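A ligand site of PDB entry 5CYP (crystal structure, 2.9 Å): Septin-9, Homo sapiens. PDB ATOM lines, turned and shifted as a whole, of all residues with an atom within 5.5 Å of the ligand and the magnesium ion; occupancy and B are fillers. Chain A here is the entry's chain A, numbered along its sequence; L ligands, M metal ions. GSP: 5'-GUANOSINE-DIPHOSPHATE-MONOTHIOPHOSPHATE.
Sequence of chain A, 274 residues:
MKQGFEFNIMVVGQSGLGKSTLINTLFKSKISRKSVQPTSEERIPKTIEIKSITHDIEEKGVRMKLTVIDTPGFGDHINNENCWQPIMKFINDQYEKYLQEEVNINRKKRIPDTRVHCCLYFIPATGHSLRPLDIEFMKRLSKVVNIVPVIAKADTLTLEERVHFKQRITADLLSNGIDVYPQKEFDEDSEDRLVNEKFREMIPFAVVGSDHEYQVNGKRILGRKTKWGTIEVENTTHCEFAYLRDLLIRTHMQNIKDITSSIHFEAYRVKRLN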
ATOM      1  N   GLY A  13     -15.207 -34.313  30.291  1.00  0.00           N
ATOM      2  CA  GLY A  13     -14.376 -33.154  30.566  1.00  0.00           C
ATOM      3  C   GLY A  13     -14.696 -32.486  31.891  1.00  0.00           C
ATOM      4  O   GLY A  13     -15.625 -32.885  32.595  1.00  0.00           O
ATOM      5  N   GLN A  14     -13.915 -31.461  32.228  1.00  0.00           N
ATOM      6  CA  GLN A  14     -14.113 -30.729  33.481  1.00  0.00           C
ATOM      7  C   GLN A  14     -15.393 -29.907  33.473  1.00  0.00           C
ATOM      8  O   GLN A  14     -16.018 -29.707  32.437  1.00  0.00           O
ATOM      9  CB  GLN A  14     -12.916 -29.811  33.757  1.00  0.00           C
ATOM     10  CG  GLN A  14     -11.737 -30.508  34.410  1.00  0.00           C
ATOM     11  CD  GLN A  14     -10.788 -29.525  35.079  1.00  0.00           C
ATOM     12  OE1 GLN A  14     -10.670 -28.384  34.648  1.00  0.00           O
ATOM     13  NE2 GLN A  14     -10.122 -29.971  36.133  1.00  0.00           N
ATOM     14  N   SER A  15     -15.771 -29.435  34.668  1.00  0.00           N
ATOM     15  CA  SER A  15     -17.012 -28.704  34.847  1.00  0.00           C
ATOM     16  C   SER A  15     -17.032 -27.364  34.111  1.00  0.00           C
ATOM     17  O   SER A  15     -16.118 -26.555  34.256  1.00  0.00           O
ATOM     18  CB  SER A  15     -17.264 -28.468  36.344  1.00  0.00           C
ATOM     19  OG  SER A  15     -17.052 -29.655  37.085  1.00  0.00           O
ATOM     20  N   GLY A  16     -18.075 -27.142  33.329  1.00  0.00           N
ATOM     21  CA  GLY A  16     -18.287 -25.867  32.675  1.00  0.00           C
ATOM     22  C   GLY A  16     -17.471 -25.652  31.408  1.00  0.00           C
ATOM     23  O   GLY A  16     -17.158 -24.518  31.070  1.00  0.00           O
ATOM     24  N   LEU A  17     -17.116 -26.736  30.738  1.00  0.00           N
ATOM     25  CA  LEU A  17     -16.328 -26.642  29.509  1.00  0.00           C
ATOM     26  C   LEU A  17     -17.195 -26.610  28.254  1.00  0.00           C
ATOM     27  O   LEU A  17     -16.673 -26.545  27.141  1.00  0.00           O
ATOM     28  CB  LEU A  17     -15.333 -27.806  29.434  1.00  0.00           C
ATOM     29  CG  LEU A  17     -14.146 -27.720  30.406  1.00  0.00           C
ATOM     30  CD1 LEU A  17     -13.183 -28.877  30.161  1.00  0.00           C
ATOM     31  CD2 LEU A  17     -13.430 -26.380  30.264  1.00  0.00           C
ATOM     32  N   GLY A  18     -18.516 -26.659  28.433  1.00  0.00           N
ATOM     33  CA  GLY A  18     -19.425 -26.573  27.320  1.00  0.00           C
ATOM     34  C   GLY A  18     -19.778 -27.931  26.722  1.00  0.00           C
ATOM     35  O   GLY A  18     -20.082 -28.034  25.541  1.00  0.00           O
ATOM     36  N   LYS A  19     -19.723 -28.963  27.561  1.00  0.00           N
ATOM     37  CA  LYS A  19     -20.028 -30.322  27.119  1.00  0.00           C
ATOM     38  C   LYS A  19     -21.492 -30.457  26.714  1.00  0.00           C
ATOM     39  O   LYS A  19     -21.804 -30.932  25.618  1.00  0.00           O
ATOM     40  CB  LYS A  19     -19.678 -31.333  28.201  1.00  0.00           C
ATOM     41  CG  LYS A  19     -18.197 -31.397  28.533  1.00  0.00           C
ATOM     42  CD  LYS A  19     -17.894 -32.541  29.487  1.00  0.00           C
ATOM     43  CE  LYS A  19     -18.708 -32.436  30.763  1.00  0.00           C
ATOM     44  NZ  LYS A  19     -17.993 -33.041  31.918  1.00  0.00           N
ATOM     45  N   SER A  20     -22.388 -30.063  27.608  1.00  0.00           N
ATOM     46  CA  SER A  20     -23.823 -30.137  27.340  1.00  0.00           C
ATOM     47  C   SER A  20     -24.215 -29.200  26.201  1.00  0.00           C
ATOM     48  O   SER A  20     -25.083 -29.514  25.391  1.00  0.00           O
ATOM     49  CB  SER A  20     -24.626 -29.799  28.594  1.00  0.00           C
ATOM     50  OG  SER A  20     -24.184 -30.560  29.700  1.00  0.00           O
ATOM     51  N   THR A  21     -23.567 -28.034  26.159  1.00  0.00           N
ATOM     52  CA  THR A  21     -23.842 -27.041  25.133  1.00  0.00           C
ATOM     53  C   THR A  21     -23.474 -27.555  23.739  1.00  0.00           C
ATOM     54  O   THR A  21     -24.134 -27.227  22.756  1.00  0.00           O
ATOM     55  CB  THR A  21     -23.075 -25.729  25.411  1.00  0.00           C
ATOM     56  OG1 THR A  21     -23.413 -25.239  26.711  1.00  0.00           O
ATOM     57  CG2 THR A  21     -23.399 -24.666  24.370  1.00  0.00           C
ATOM     58  N   LEU A  22     -22.447 -28.407  23.669  1.00  0.00           N
ATOM     59  CA  LEU A  22     -22.016 -28.944  22.389  1.00  0.00           C
ATOM     60  C   LEU A  22     -22.987 -30.020  21.913  1.00  0.00           C
ATOM     61  O   LEU A  22     -23.150 -30.227  20.706  1.00  0.00           O
ATOM     62  CB  LEU A  22     -20.607 -29.521  22.489  1.00  0.00           C
ATOM     63  CG  LEU A  22     -19.914 -29.757  21.143  1.00  0.00           C
ATOM     64  CD1 LEU A  22     -19.360 -28.448  20.594  1.00  0.00           C
ATOM     65  CD2 LEU A  22     -18.820 -30.807  21.245  1.00  0.00           C
ATOM     66  N   ILE A  44     -28.704 -23.927  30.371  1.00  0.00           N
ATOM     67  CA  ILE A  44     -28.558 -25.371  30.504  1.00  0.00           C
ATOM     68  C   ILE A  44     -28.147 -25.682  31.935  1.00  0.00           C
ATOM     69  O   ILE A  44     -27.119 -25.206  32.407  1.00  0.00           O
ATOM     70  CB  ILE A  44     -27.509 -25.934  29.530  1.00  0.00           C
ATOM     71  CG1 ILE A  44     -27.915 -25.652  28.084  1.00  0.00           C
ATOM     72  CG2 ILE A  44     -27.338 -27.437  29.755  1.00  0.00           C
ATOM     73  CD1 ILE A  44     -26.980 -26.262  27.063  1.00  0.00           C
ATOM     74  N   PRO A  45     -28.964 -26.474  32.645  1.00  0.00           N
ATOM     75  CA  PRO A  45     -28.700 -26.761  34.054  1.00  0.00           C
ATOM     76  C   PRO A  45     -27.407 -27.548  34.267  1.00  0.00           C
ATOM     77  O   PRO A  45     -26.853 -28.107  33.312  1.00  0.00           O
ATOM     78  CB  PRO A  45     -29.918 -27.584  34.492  1.00  0.00           C
ATOM     79  CG  PRO A  45     -30.421 -28.204  33.225  1.00  0.00           C
ATOM     80  CD  PRO A  45     -30.176 -27.180  32.161  1.00  0.00           C
ATOM     81  N   LYS A  46     -26.944 -27.596  35.501  1.00  0.00           N
ATOM     82  CA  LYS A  46     -25.736 -28.331  35.857  1.00  0.00           C
ATOM     83  C   LYS A  46     -25.961 -29.833  35.739  1.00  0.00           C
ATOM     84  O   LYS A  46     -26.887 -30.383  36.336  1.00  0.00           O
ATOM     85  CB  LYS A  46     -25.292 -27.948  37.277  1.00  0.00           C
ATOM     86  CG  LYS A  46     -24.052 -28.656  37.778  1.00  0.00           C
ATOM     87  CD  LYS A  46     -23.469 -27.959  39.005  1.00  0.00           C
ATOM     88  CE  LYS A  46     -24.530 -27.725  40.080  1.00  0.00           C
ATOM     89  NZ  LYS A  46     -25.394 -26.535  39.796  1.00  0.00           N
ATOM     90  N   THR A  47     -25.088 -30.499  34.978  1.00  0.00           N
ATOM     91  CA  THR A  47     -25.213 -31.931  34.760  1.00  0.00           C
ATOM     92  C   THR A  47     -24.768 -32.715  35.986  1.00  0.00           C
ATOM     93  O   THR A  47     -23.577 -32.780  36.283  1.00  0.00           O
ATOM     94  CB  THR A  47     -24.395 -32.387  33.542  1.00  0.00           C
ATOM     95  OG1 THR A  47     -24.657 -31.517  32.433  1.00  0.00           O
ATOM     96  CG2 THR A  47     -24.754 -33.816  33.154  1.00  0.00           C
ATOM     97  N   ASP A  70     -24.162 -37.544  28.023  1.00  0.00           N
ATOM     98  CA  ASP A  70     -23.653 -36.411  28.776  1.00  0.00           C
ATOM     99  C   ASP A  70     -23.120 -36.871  30.129  1.00  0.00           C
ATOM    100  O   ASP A  70     -23.716 -37.746  30.774  1.00  0.00           O
ATOM    101  CB  ASP A  70     -24.741 -35.351  28.973  1.00  0.00           C
ATOM    102  CG  ASP A  70     -24.171 -33.997  29.323  1.00  0.00           C
ATOM    103  OD1 ASP A  70     -22.957 -33.794  29.147  1.00  0.00           O
ATOM    104  OD2 ASP A  70     -24.946 -33.127  29.782  1.00  0.00           O
ATOM    105  N   THR A  71     -22.011 -36.282  30.565  1.00  0.00           N
ATOM    106  CA  THR A  71     -21.394 -36.665  31.831  1.00  0.00           C
ATOM    107  C   THR A  71     -21.191 -35.449  32.740  1.00  0.00           C
ATOM    108  O   THR A  71     -20.931 -34.349  32.257  1.00  0.00           O
ATOM    109  CB  THR A  71     -20.038 -37.360  31.616  1.00  0.00           C
ATOM    110  OG1 THR A  71     -19.147 -36.466  30.935  1.00  0.00           O
ATOM    111  CG2 THR A  71     -20.211 -38.630  30.789  1.00  0.00           C
ATOM    112  N   PRO A  72     -21.302 -35.661  34.060  1.00  0.00           N
ATOM    113  CA  PRO A  72     -20.998 -34.603  35.036  1.00  0.00           C
ATOM    114  C   PRO A  72     -19.512 -34.255  35.016  1.00  0.00           C
ATOM    115  O   PRO A  72     -18.675 -35.160  34.952  1.00  0.00           O
ATOM    116  CB  PRO A  72     -21.413 -35.217  36.366  1.00  0.00           C
ATOM    117  CG  PRO A  72     -21.367 -36.689  36.145  1.00  0.00           C
ATOM    118  CD  PRO A  72     -21.772 -36.887  34.718  1.00  0.00           C
ATOM    119  N   GLY A  73     -19.194 -32.965  35.093  1.00  0.00           N
ATOM    120  CA  GLY A  73     -17.810 -32.520  35.062  1.00  0.00           C
ATOM    121  C   GLY A  73     -17.005 -32.987  36.261  1.00  0.00           C
ATOM    122  O   GLY A  73     -17.534 -33.166  37.351  1.00  0.00           O
ATOM    123  N   LYS A 153     -14.331 -24.488  24.402  1.00  0.00           N
ATOM    124  CA  LYS A 153     -14.453 -23.044  24.274  1.00  0.00           C
ATOM    125  C   LYS A 153     -13.282 -22.438  23.508  1.00  0.00           C
ATOM    126  O   LYS A 153     -12.519 -21.654  24.051  1.00  0.00           O
ATOM    127  CB  LYS A 153     -14.572 -22.391  25.652  1.00  0.00           C
ATOM    128  CG  LYS A 153     -15.776 -22.863  26.448  1.00  0.00           C
ATOM    129  CD  LYS A 153     -15.774 -22.292  27.859  1.00  0.00           C
ATOM    130  CE  LYS A 153     -17.087 -22.570  28.567  1.00  0.00           C
ATOM    131  NZ  LYS A 153     -17.142 -21.939  29.914  1.00  0.00           N
ATOM    132  N   ALA A 154     -13.149 -22.818  22.234  1.00  0.00           N
ATOM    133  CA  ALA A 154     -12.017 -22.398  21.415  1.00  0.00           C
ATOM    134  C   ALA A 154     -12.060 -20.917  21.075  1.00  0.00           C
ATOM    135  O   ALA A 154     -11.095 -20.363  20.554  1.00  0.00           O
ATOM    136  CB  ALA A 154     -11.967 -23.225  20.138  1.00  0.00           C
ATOM    137  N   ASP A 155     -13.185 -20.265  21.364  1.00  0.00           N
ATOM    138  CA  ASP A 155     -13.323 -18.824  21.167  1.00  0.00           C
ATOM    139  C   ASP A 155     -12.556 -18.043  22.230  1.00  0.00           C
ATOM    140  O   ASP A 155     -12.356 -16.840  22.105  1.00  0.00           O
ATOM    141  CB  ASP A 155     -14.793 -18.429  21.157  1.00  0.00           C
ATOM    142  CG  ASP A 155     -15.554 -18.949  22.363  1.00  0.00           C
ATOM    143  OD1 ASP A 155     -15.236 -20.073  22.820  1.00  0.00           O
ATOM    144  OD2 ASP A 155     -16.450 -18.242  22.866  1.00  0.00           O
ATOM    145  N   THR A 156     -12.143 -18.742  23.290  1.00  0.00           N
ATOM    146  CA  THR A 156     -11.351 -18.152  24.360  1.00  0.00           C
ATOM    147  C   THR A 156      -9.990 -17.696  23.838  1.00  0.00           C
ATOM    148  O   THR A 156      -9.451 -16.666  24.273  1.00  0.00           O
ATOM    149  CB  THR A 156     -11.146 -19.149  25.511  1.00  0.00           C
ATOM    150  OG1 THR A 156     -12.420 -19.612  25.977  1.00  0.00           O
ATOM    151  CG2 THR A 156     -10.387 -18.514  26.666  1.00  0.00           C
ATOM    152  N   VAL A 207     -13.550 -26.612  19.096  1.00  0.00           N
ATOM    153  CA  VAL A 207     -15.006 -26.517  19.003  1.00  0.00           C
ATOM    154  C   VAL A 207     -15.552 -25.314  19.762  1.00  0.00           C
ATOM    155  O   VAL A 207     -14.906 -24.782  20.669  1.00  0.00           O
ATOM    156  CB  VAL A 207     -15.697 -27.787  19.526  1.00  0.00           C
ATOM    157  CG1 VAL A 207     -15.093 -29.021  18.890  1.00  0.00           C
ATOM    158  CG2 VAL A 207     -15.598 -27.854  21.041  1.00  0.00           C
ATOM    159  N   VAL A 208     -16.754 -24.891  19.387  1.00  0.00           N
ATOM    160  CA  VAL A 208     -17.442 -23.793  20.052  1.00  0.00           C
ATOM    161  C   VAL A 208     -18.925 -24.108  20.191  1.00  0.00           C
ATOM    162  O   VAL A 208     -19.597 -24.403  19.193  1.00  0.00           O
ATOM    163  CB  VAL A 208     -17.275 -22.456  19.300  1.00  0.00           C
ATOM    164  CG1 VAL A 208     -18.192 -21.386  19.894  1.00  0.00           C
ATOM    165  CG2 VAL A 208     -15.824 -21.994  19.334  1.00  0.00           C
ATOM    166  N   GLY A 209     -19.438 -24.056  21.416  1.00  0.00           N
ATOM    167  CA  GLY A 209     -20.853 -24.289  21.654  1.00  0.00           C
ATOM    168  C   GLY A 209     -21.688 -23.150  21.104  1.00  0.00           C
ATOM    169  O   GLY A 209     -21.219 -22.018  21.009  1.00  0.00           O
ATOM    170  N   SER A 210     -22.938 -23.442  20.753  1.00  0.00           N
ATOM    171  CA  SER A 210     -23.807 -22.440  20.138  1.00  0.00           C
ATOM    172  C   SER A 210     -24.685 -21.737  21.171  1.00  0.00           C
ATOM    173  O   SER A 210     -25.531 -22.362  21.809  1.00  0.00           O
ATOM    174  CB  SER A 210     -24.685 -23.082  19.065  1.00  0.00           C
ATOM    175  OG  SER A 210     -25.609 -23.987  19.631  1.00  0.00           O
ATOM    176  N   ARG A 224     -22.404 -17.604  18.339  1.00  0.00           N
ATOM    177  CA  ARG A 224     -21.846 -17.364  19.661  1.00  0.00           C
ATOM    178  C   ARG A 224     -21.424 -15.907  19.790  1.00  0.00           C
ATOM    179  O   ARG A 224     -20.513 -15.445  19.097  1.00  0.00           O
ATOM    180  CB  ARG A 224     -20.646 -18.286  19.907  1.00  0.00           C
ATOM    181  CG  ARG A 224     -20.076 -18.206  21.315  1.00  0.00           C
ATOM    182  CD  ARG A 224     -20.962 -18.941  22.297  1.00  0.00           C
ATOM    183  NE  ARG A 224     -20.681 -18.570  23.680  1.00  0.00           N
ATOM    184  CZ  ARG A 224     -21.261 -19.119  24.744  1.00  0.00           C
ATOM    185  NH1 ARG A 224     -20.946 -18.710  25.962  1.00  0.00           N
ATOM    186  NH2 ARG A 224     -22.150 -20.091  24.574  1.00  0.00           N
HETATM  187  PG  GSP L   1     -21.001 -29.113  33.517  1.00  0.00           P
HETATM  188  O3B GSP L   1     -21.025 -27.803  32.739  1.00  0.00           O
HETATM  189  S1G GSP L   1     -21.265 -29.212  35.374  1.00  0.00           S
HETATM  190  O2G GSP L   1     -22.110 -30.024  32.792  1.00  0.00           O
HETATM  191  O3G GSP L   1     -19.731 -29.912  32.984  1.00  0.00           O
HETATM  192  PB  GSP L   1     -20.894 -28.119  31.033  1.00  0.00           P
HETATM  193  O1B GSP L   1     -19.672 -28.968  31.169  1.00  0.00           O
HETATM  194  O2B GSP L   1     -22.264 -28.693  30.814  1.00  0.00           O
HETATM  195  PA  GSP L   1     -22.219 -26.180  29.960  1.00  0.00           P
HETATM  196  O1A GSP L   1     -22.703 -26.071  31.377  1.00  0.00           O
HETATM  197  O2A GSP L   1     -22.962 -26.960  28.903  1.00  0.00           O
HETATM  198  O3A GSP L   1     -20.759 -26.823  30.165  1.00  0.00           O
HETATM  199  O5' GSP L   1     -21.987 -24.642  29.470  1.00  0.00           O
HETATM  200  C5' GSP L   1     -21.405 -24.034  30.579  1.00  0.00           C
HETATM  201  C4' GSP L   1     -21.236 -22.578  30.206  1.00  0.00           C
HETATM  202  O4' GSP L   1     -20.255 -22.516  29.148  1.00  0.00           O
HETATM  203  C3' GSP L   1     -22.560 -21.987  29.650  1.00  0.00           C
HETATM  204  O3' GSP L   1     -22.764 -20.747  30.242  1.00  0.00           O
HETATM  205  C2' GSP L   1     -22.280 -21.848  28.149  1.00  0.00           C
HETATM  206  O2' GSP L   1     -22.834 -20.696  27.606  1.00  0.00           O
HETATM  207  C1' GSP L   1     -20.744 -21.654  28.147  1.00  0.00           C
HETATM  208  N9  GSP L   1     -20.190 -22.145  26.909  1.00  0.00           N
HETATM  209  C8  GSP L   1     -20.473 -23.396  26.273  1.00  0.00           C
HETATM  210  N7  GSP L   1     -19.778 -23.527  25.134  1.00  0.00           N
HETATM  211  C5  GSP L   1     -19.046 -22.348  25.030  1.00  0.00           C
HETATM  212  C6  GSP L   1     -18.151 -22.004  23.977  1.00  0.00           C
HETATM  213  O6  GSP L   1     -17.835 -22.633  22.986  1.00  0.00           O
HETATM  214  N1  GSP L   1     -17.552 -20.719  24.176  1.00  0.00           N
HETATM  215  C2  GSP L   1     -17.862 -19.937  25.302  1.00  0.00           C
HETATM  216  N2  GSP L   1     -17.231 -18.711  25.386  1.00  0.00           N
HETATM  217  N3  GSP L   1     -18.709 -20.231  26.312  1.00  0.00           N
HETATM  218  C4  GSP L   1     -19.280 -21.488  26.102  1.00  0.00           C
HETATM  219 MG    MG M   1     -22.980 -30.852  31.225  1.00  0.00          MG
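The side-chain amino group (NZ) of Lys 19 lies within hydrogen-bond range of the backbone carbonyl oxygen (O) of Gly 13 (2.5 Å).
The backbone carbonyl oxygen (O) of Gly 16 sits at hydrogen-bond distance from the side-chain amino group (NZ) of Lys 153.
NZ of Lys 19 lies within hydrogen-bond range of O of Thr 71 (3.2 Å).
The side-chain carboxylate (OD2) of Asp 70 lies close to the side-chain hydroxyl (OG1) of Thr 47 (3.1 Å).
The side-chain hydroxyl (OG) of Ser 20 sits close to the side-chain carboxylate (OD2) of Asp 70, 2.7 Å away.
The side-chain hydroxyl (OG1) of Thr 156 sits at hydrogen-bond distance from the backbone carbonyl oxygen (O) of Lys 153, at 2.8 Å.
O3A of the ligand lies within hydrogen-bond range of N of Gly 18, 2.8 Å away.
The guanidinium group of Arg 224 lies within hydrogen-bond range of a nitrogen (N3) of the ligand.
An oxygen (O1B) of the ligand lies within hydrogen-bond range of the backbone NH (N) of Leu 17 (3.4 Å).
N of Ser 20 sits close to O2A of the ligand (3.4 Å).
An oxygen (O6) of the ligand is in hydrogen-bond range of the backbone NH (N) of Gly 209.
O2A of the ligand sits at hydrogen-bond distance from OG1 of Thr 21 (2.8 Å).
NZ of Lys 153 lies close to O4' of the ligand (3.3 Å).
N of Thr 21 sits at hydrogen-bond distance from O2A of the ligand.
An oxygen (O3B) of the ligand sits at hydrogen-bond distance from the backbone NH (N) of Gly 16 (3.1 Å).
A nitrogen (N2) of the ligand is in hydrogen-bond range of the side-chain carboxylate (OD2) of Asp 155 (2.7 Å).
OG of Ser 20 binds the magnesium ion (2.0 Å).
O2G of the ligand is bound to the magnesium ion (2.0 Å).
OG1 of Thr 47 binds the magnesium ion (2.2 Å).
The magnesium ion is bound by O2B of the ligand (2.3 Å).
The magnesium ion has four donor atoms within binding distance.
Merely in contact with the ligand: Val 208 (3.2 Å), Ser 15 (3.5 Å), Lys 19 (3.5 Å), Lys 46 (3.7 Å), Gly 73 (3.7 Å) and Gln 14 (3.8 Å).
Hydrophobic or aromatic side chains that line the ligand: Val 208.
Of the 27 residues printed, 16 come within 4 Å of the ligand.
Along chain A the residues within 4 Å of the ligand span positions 14 to 224.
The nearest printed residue that does not touch the ligand is Val 207 (4.3 Å).
Asp 70 touches the magnesium ion (OD2 to MG, 3.3 Å).
Within 4 Å of the magnesium ion: Ser 20, Thr 47 and Asp 70.
The nearest printed residue that does not touch the magnesium ion is Thr 71 (4.2 Å).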
